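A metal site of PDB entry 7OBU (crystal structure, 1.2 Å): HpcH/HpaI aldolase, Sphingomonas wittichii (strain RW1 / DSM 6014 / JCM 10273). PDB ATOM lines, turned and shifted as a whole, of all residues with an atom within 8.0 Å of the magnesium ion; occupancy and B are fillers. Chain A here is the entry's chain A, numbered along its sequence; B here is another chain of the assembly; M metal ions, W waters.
Water W3 bridges the side-chain carboxylate (OE2) of Glu 146 and the side-chain amide nitrogen (NE2) of Gln 44.
Residues that only touch the magnesium ion: Gln 44 (3.99 Å).
Of the 21 residues printed, 4 come within 4 Å of the magnesium ion.
The nearest printed residue that does not touch the magnesium ion is His 45 (4.2 Å).
The magnesium ion is bound by OD2 of Asp 172, water W2, OE1 of Glu 146, water W3, OG of Ser 117 of chain B and water W1.
The side-chain amide oxygen (OE1) of Gln 44 sits close to the guanidinium group (NE) of Arg 70.
The side-chain carboxylate of Asp 172 lies within hydrogen-bond range of the backbone NH of Phe 118 of chain B (2.8 Å).
The backbone NH of Ser 117 of chain B lies within hydrogen-bond range of the side-chain sulfur of Met 80 of chain B (3.4 Å).
The backbone NH (N) of Met 94 is in hydrogen-bond range of the side-chain carboxylate (OE2) of Glu 146, 2.8 Å away.
OG of Ser 117 of chain B lies close to NE2 of His 45 (2.6 Å).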
ATOM      1  N   GLN A  44     -11.941 -20.777 -20.491  1.00  0.00           N
ATOM      2  CA  GLN A  44     -11.157 -20.423 -19.322  1.00  0.00           C
ATOM      3  C   GLN A  44     -11.255 -18.922 -19.048  1.00  0.00           C
ATOM      4  O   GLN A  44     -11.780 -18.515 -18.013  1.00  0.00           O
ATOM      5  CB  GLN A  44      -9.706 -20.885 -19.551  1.00  0.00           C
ATOM      6  CG  GLN A  44      -8.780 -20.595 -18.356  1.00  0.00           C
ATOM      7  CD  GLN A  44      -7.331 -20.949 -18.624  1.00  0.00           C
ATOM      8  OE1 GLN A  44      -6.809 -20.707 -19.730  1.00  0.00           O
ATOM      9  NE2 GLN A  44      -6.659 -21.480 -17.619  1.00  0.00           N
ATOM     10  N   HIS A  45     -10.771 -18.098 -19.965  1.00  0.00           N
ATOM     11  CA  HIS A  45     -10.726 -16.640 -19.800  1.00  0.00           C
ATOM     12  C   HIS A  45     -11.859 -15.959 -20.556  1.00  0.00           C
ATOM     13  O   HIS A  45     -11.667 -15.128 -21.462  1.00  0.00           O
ATOM     14  CB  HIS A  45      -9.347 -16.107 -20.153  1.00  0.00           C
ATOM     15  CG  HIS A  45      -8.302 -16.575 -19.202  1.00  0.00           C
ATOM     16  ND1 HIS A  45      -8.291 -16.175 -17.876  1.00  0.00           N
ATOM     17  CD2 HIS A  45      -7.290 -17.449 -19.340  1.00  0.00           C
ATOM     18  CE1 HIS A  45      -7.284 -16.778 -17.250  1.00  0.00           C
ATOM     19  NE2 HIS A  45      -6.650 -17.537 -18.126  1.00  0.00           N
ATOM     20  N   ARG A  70     -10.614 -24.736 -25.667  1.00  0.00           N
ATOM     21  CA  ARG A  70      -9.598 -24.565 -24.640  1.00  0.00           C
ATOM     22  C   ARG A  70     -10.329 -24.636 -23.311  1.00  0.00           C
ATOM     23  O   ARG A  70     -11.131 -23.749 -22.978  1.00  0.00           O
ATOM     24  CB  ARG A  70      -8.819 -23.266 -24.796  1.00  0.00           C
ATOM     25  CG  ARG A  70      -7.598 -23.159 -23.873  1.00  0.00           C
ATOM     26  CD  ARG A  70      -7.902 -22.463 -22.573  1.00  0.00           C
ATOM     27  NE  ARG A  70      -7.969 -21.010 -22.736  1.00  0.00           N
ATOM     28  CZ  ARG A  70      -6.925 -20.189 -22.775  1.00  0.00           C
ATOM     29  NH1 ARG A  70      -5.695 -20.646 -22.822  1.00  0.00           N
ATOM     30  NH2 ARG A  70      -7.133 -18.875 -22.733  1.00  0.00           N
ATOM     31  N   GLN A  72     -11.266 -25.037 -19.176  1.00  0.00           N
ATOM     32  CA  GLN A  72     -10.808 -24.297 -18.009  1.00  0.00           C
ATOM     33  C   GLN A  72      -9.786 -25.087 -17.201  1.00  0.00           C
ATOM     34  O   GLN A  72      -8.988 -24.489 -16.471  1.00  0.00           O
ATOM     35  CB  GLN A  72     -11.968 -23.828 -17.125  1.00  0.00           C
ATOM     36  CG  GLN A  72     -12.391 -24.793 -16.125  1.00  0.00           C
ATOM     37  CD  GLN A  72     -13.421 -24.240 -15.172  1.00  0.00           C
ATOM     38  OE1 GLN A  72     -14.459 -23.690 -15.577  1.00  0.00           O
ATOM     39  NE2 GLN A  72     -13.169 -24.412 -13.876  1.00  0.00           N
ATOM     40  N   PRO A  93      -5.306 -26.578 -20.141  1.00  0.00           N
ATOM     41  CA  PRO A  93      -4.340 -25.741 -19.424  1.00  0.00           C
ATOM     42  C   PRO A  93      -3.500 -26.496 -18.403  1.00  0.00           C
ATOM     43  O   PRO A  93      -3.879 -27.558 -17.893  1.00  0.00           O
ATOM     44  CB  PRO A  93      -5.213 -24.730 -18.680  1.00  0.00           C
ATOM     45  CG  PRO A  93      -6.564 -24.921 -19.068  1.00  0.00           C
ATOM     46  CD  PRO A  93      -6.696 -26.226 -19.798  1.00  0.00           C
ATOM     47  N   MET A  94      -2.385 -25.852 -18.032  1.00  0.00           N
ATOM     48  CA  MET A  94      -1.581 -26.244 -16.879  1.00  0.00           C
ATOM     49  C   MET A  94      -1.121 -27.692 -16.954  1.00  0.00           C
ATOM     50  O   MET A  94      -1.154 -28.446 -15.968  1.00  0.00           O
ATOM     51  CB  MET A  94      -2.306 -25.987 -15.550  1.00  0.00           C
ATOM     52  CG  MET A  94      -2.523 -24.527 -15.293  1.00  0.00           C
ATOM     53  SD  MET A  94      -0.976 -23.703 -14.886  1.00  0.00           S
ATOM     54  CE  MET A  94      -0.794 -24.193 -13.157  1.00  0.00           C
ATOM     55  N   MET A 144      -1.255 -27.551 -22.901  1.00  0.00           N
ATOM     56  CA  MET A 144      -0.741 -26.200 -22.818  1.00  0.00           C
ATOM     57  C   MET A 144       0.570 -26.160 -22.054  1.00  0.00           C
ATOM     58  O   MET A 144       0.715 -26.789 -20.991  1.00  0.00           O
ATOM     59  CB  MET A 144      -1.718 -25.266 -22.138  1.00  0.00           C
ATOM     60  CG  MET A 144      -2.898 -24.902 -22.992  1.00  0.00           C
ATOM     61  SD  MET A 144      -4.060 -23.796 -22.172  1.00  0.00           S
ATOM     62  CE  MET A 144      -2.972 -22.425 -21.835  1.00  0.00           C
ATOM     63  N   ILE A 145       1.490 -25.355 -22.568  1.00  0.00           N
ATOM     64  CA  ILE A 145       2.790 -25.065 -21.967  1.00  0.00           C
ATOM     65  C   ILE A 145       2.765 -23.579 -21.630  1.00  0.00           C
ATOM     66  O   ILE A 145       2.781 -22.728 -22.529  1.00  0.00           O
ATOM     67  CB  ILE A 145       3.917 -25.378 -22.944  1.00  0.00           C
ATOM     68  CG1 ILE A 145       3.845 -26.839 -23.379  1.00  0.00           C
ATOM     69  CG2 ILE A 145       5.277 -25.039 -22.325  1.00  0.00           C
ATOM     70  CD1 ILE A 145       4.035 -27.829 -22.240  1.00  0.00           C
ATOM     71  N   GLU A 146       2.642 -23.275 -20.335  1.00  0.00           N
ATOM     72  CA  GLU A 146       2.397 -21.908 -19.907  1.00  0.00           C
ATOM     73  C   GLU A 146       3.065 -21.617 -18.562  1.00  0.00           C
ATOM     74  O   GLU A 146       2.757 -20.599 -17.924  1.00  0.00           O
ATOM     75  CB  GLU A 146       0.889 -21.620 -19.900  1.00  0.00           C
ATOM     76  CG  GLU A 146       0.103 -22.594 -19.074  1.00  0.00           C
ATOM     77  CD  GLU A 146      -1.335 -22.203 -18.831  1.00  0.00           C
ATOM     78  OE1 GLU A 146      -1.669 -20.998 -18.960  1.00  0.00           O
ATOM     79  OE2 GLU A 146      -2.136 -23.105 -18.464  1.00  0.00           O
ATOM     80  N   THR A 147       3.994 -22.460 -18.123  1.00  0.00           N
ATOM     81  CA  THR A 147       4.682 -22.254 -16.858  1.00  0.00           C
ATOM     82  C   THR A 147       6.158 -22.592 -17.022  1.00  0.00           C
ATOM     83  O   THR A 147       6.562 -23.322 -17.923  1.00  0.00           O
ATOM     84  CB  THR A 147       4.133 -23.117 -15.715  1.00  0.00           C
ATOM     85  OG1 THR A 147       4.406 -24.489 -16.018  1.00  0.00           O
ATOM     86  CG2 THR A 147       2.633 -22.942 -15.505  1.00  0.00           C
ATOM     87  N   GLY A 169       1.131 -20.830 -24.457  1.00  0.00           N
ATOM     88  CA  GLY A 169       0.482 -19.599 -24.065  1.00  0.00           C
ATOM     89  C   GLY A 169       1.514 -18.553 -23.664  1.00  0.00           C
ATOM     90  O   GLY A 169       1.991 -18.546 -22.520  1.00  0.00           O
ATOM     91  N   THR A 171       1.689 -15.283 -23.014  1.00  0.00           N
ATOM     92  CA  THR A 171       1.491 -14.271 -21.986  1.00  0.00           C
ATOM     93  C   THR A 171       1.629 -14.868 -20.587  1.00  0.00           C
ATOM     94  O   THR A 171       2.293 -14.289 -19.717  1.00  0.00           O
ATOM     95  CB  THR A 171       0.120 -13.611 -22.178  1.00  0.00           C
ATOM     96  OG1 THR A 171       0.042 -13.037 -23.480  1.00  0.00           O
ATOM     97  CG2 THR A 171      -0.131 -12.572 -21.099  1.00  0.00           C
ATOM     98  N   ASP A 172       0.996 -16.016 -20.342  1.00  0.00           N
ATOM     99  CA  ASP A 172       1.133 -16.674 -19.051  1.00  0.00           C
ATOM    100  C   ASP A 172       2.561 -17.155 -18.834  1.00  0.00           C
ATOM    101  O   ASP A 172       3.052 -17.137 -17.702  1.00  0.00           O
ATOM    102  CB  ASP A 172       0.185 -17.855 -18.932  1.00  0.00           C
ATOM    103  CG  ASP A 172      -1.139 -17.495 -18.287  1.00  0.00           C
ATOM    104  OD1 ASP A 172      -1.201 -16.595 -17.407  1.00  0.00           O
ATOM    105  OD2 ASP A 172      -2.123 -18.202 -18.658  1.00  0.00           O
ATOM    106  N   LEU A 173       3.228 -17.612 -19.895  1.00  0.00           N
ATOM    107  CA  LEU A 173       4.604 -18.043 -19.739  1.00  0.00           C
ATOM    108  C   LEU A 173       5.457 -16.855 -19.308  1.00  0.00           C
ATOM    109  O   LEU A 173       6.283 -16.975 -18.400  1.00  0.00           O
ATOM    110  CB  LEU A 173       5.095 -18.641 -21.051  1.00  0.00           C
ATOM    111  CG  LEU A 173       6.492 -19.245 -21.025  1.00  0.00           C
ATOM    112  CD1 LEU A 173       6.600 -20.369 -20.020  1.00  0.00           C
ATOM    113  CD2 LEU A 173       6.844 -19.738 -22.393  1.00  0.00           C
ATOM    114  N   LEU A 175       4.503 -14.180 -17.698  1.00  0.00           N
ATOM    115  CA  LEU A 175       4.150 -13.802 -16.335  1.00  0.00           C
ATOM    116  C   LEU A 175       4.788 -14.771 -15.355  1.00  0.00           C
ATOM    117  O   LEU A 175       5.359 -14.367 -14.331  1.00  0.00           O
ATOM    118  CB  LEU A 175       2.631 -13.786 -16.218  1.00  0.00           C
ATOM    119  CG  LEU A 175       1.996 -13.417 -14.879  1.00  0.00           C
ATOM    120  CD1 LEU A 175       2.490 -12.073 -14.343  1.00  0.00           C
ATOM    121  CD2 LEU A 175       0.473 -13.403 -15.002  1.00  0.00           C
ATOM    122  N   MET B  80     -10.565 -18.885 -10.518  1.00  0.00           N
ATOM    123  CA  MET B  80      -9.994 -17.982 -11.524  1.00  0.00           C
ATOM    124  C   MET B  80     -11.056 -17.508 -12.507  1.00  0.00           C
ATOM    125  O   MET B  80     -11.061 -16.338 -12.920  1.00  0.00           O
ATOM    126  CB  MET B  80      -8.864 -18.684 -12.242  1.00  0.00           C
ATOM    127  CG  MET B  80      -7.641 -18.902 -11.397  1.00  0.00           C
ATOM    128  SD  MET B  80      -6.364 -19.767 -12.338  1.00  0.00           S
ATOM    129  CE  MET B  80      -5.520 -20.720 -11.110  1.00  0.00           C
ATOM    130  N   LEU B 115      -0.463 -18.460  -8.730  1.00  0.00           N
ATOM    131  CA  LEU B 115      -0.422 -19.007 -10.075  1.00  0.00           C
ATOM    132  C   LEU B 115      -1.666 -18.660 -10.883  1.00  0.00           C
ATOM    133  O   LEU B 115      -2.005 -19.373 -11.822  1.00  0.00           O
ATOM    134  CB  LEU B 115      -0.145 -20.519 -10.085  1.00  0.00           C
ATOM    135  CG  LEU B 115      -0.972 -21.382  -9.139  1.00  0.00           C
ATOM    136  CD1 LEU B 115      -2.439 -21.401  -9.550  1.00  0.00           C
ATOM    137  CD2 LEU B 115      -0.366 -22.792  -9.062  1.00  0.00           C
ATOM    138  N   ARG B 116      -2.319 -17.554 -10.549  1.00  0.00           N
ATOM    139  CA  ARG B 116      -3.525 -17.148 -11.247  1.00  0.00           C
ATOM    140  C   ARG B 116      -3.237 -16.983 -12.731  1.00  0.00           C
ATOM    141  O   ARG B 116      -2.279 -16.319 -13.124  1.00  0.00           O
ATOM    142  CB  ARG B 116      -4.031 -15.829 -10.670  1.00  0.00           C
ATOM    143  CG  ARG B 116      -5.297 -15.339 -11.311  1.00  0.00           C
ATOM    144  CD  ARG B 116      -5.771 -14.022 -10.747  1.00  0.00           C
ATOM    145  NE  ARG B 116      -6.889 -13.509 -11.525  1.00  0.00           N
ATOM    146  CZ  ARG B 116      -7.283 -12.248 -11.492  1.00  0.00           C
ATOM    147  NH1 ARG B 116      -6.735 -11.378 -10.677  1.00  0.00           N
ATOM    148  NH2 ARG B 116      -8.286 -11.849 -12.274  1.00  0.00           N
ATOM    149  N   SER B 117      -4.078 -17.596 -13.559  1.00  0.00           N
ATOM    150  CA  SER B 117      -3.933 -17.517 -15.000  1.00  0.00           C
ATOM    151  C   SER B 117      -4.394 -16.150 -15.504  1.00  0.00           C
ATOM    152  O   SER B 117      -5.342 -15.566 -14.974  1.00  0.00           O
ATOM    153  CB  SER B 117      -4.770 -18.610 -15.629  1.00  0.00           C
ATOM    154  OG  SER B 117      -4.564 -18.732 -17.028  1.00  0.00           O
ATOM    155  N   PHE B 118      -3.736 -15.653 -16.549  1.00  0.00           N
ATOM    156  CA  PHE B 118      -3.950 -14.300 -17.018  1.00  0.00           C
ATOM    157  C   PHE B 118      -5.001 -14.192 -18.115  1.00  0.00           C
ATOM    158  O   PHE B 118      -4.817 -14.717 -19.233  1.00  0.00           O
ATOM    159  CB  PHE B 118      -2.668 -13.654 -17.533  1.00  0.00           C
ATOM    160  CG  PHE B 118      -2.830 -12.200 -17.782  1.00  0.00           C
ATOM    161  CD1 PHE B 118      -2.807 -11.310 -16.723  1.00  0.00           C
ATOM    162  CD2 PHE B 118      -3.102 -11.713 -19.046  1.00  0.00           C
ATOM    163  CE1 PHE B 118      -3.000  -9.949 -16.927  1.00  0.00           C
ATOM    164  CE2 PHE B 118      -3.295 -10.352 -19.250  1.00  0.00           C
ATOM    165  CZ  PHE B 118      -3.239  -9.485 -18.182  1.00  0.00           C
ATOM    166  N   GLY B 119      -6.055 -13.446 -17.839  1.00  0.00           N
ATOM    167  CA  GLY B 119      -7.027 -13.068 -18.830  1.00  0.00           C
ATOM    168  C   GLY B 119      -8.187 -12.392 -18.155  1.00  0.00           C
ATOM    169  O   GLY B 119      -9.307 -12.934 -18.096  1.00  0.00           O
HETATM  170 MG    MG M   1      -3.066 -19.802 -18.025  1.00  0.00          MG
HETATM  171  O   HOH W   1      -1.900 -19.855 -16.258  1.00  0.00           O
HETATM  172  O   HOH W   2      -4.281 -19.746 -19.660  1.00  0.00           O
HETATM  173  O   HOH W   3      -3.889 -21.561 -17.294  1.00  0.00           O
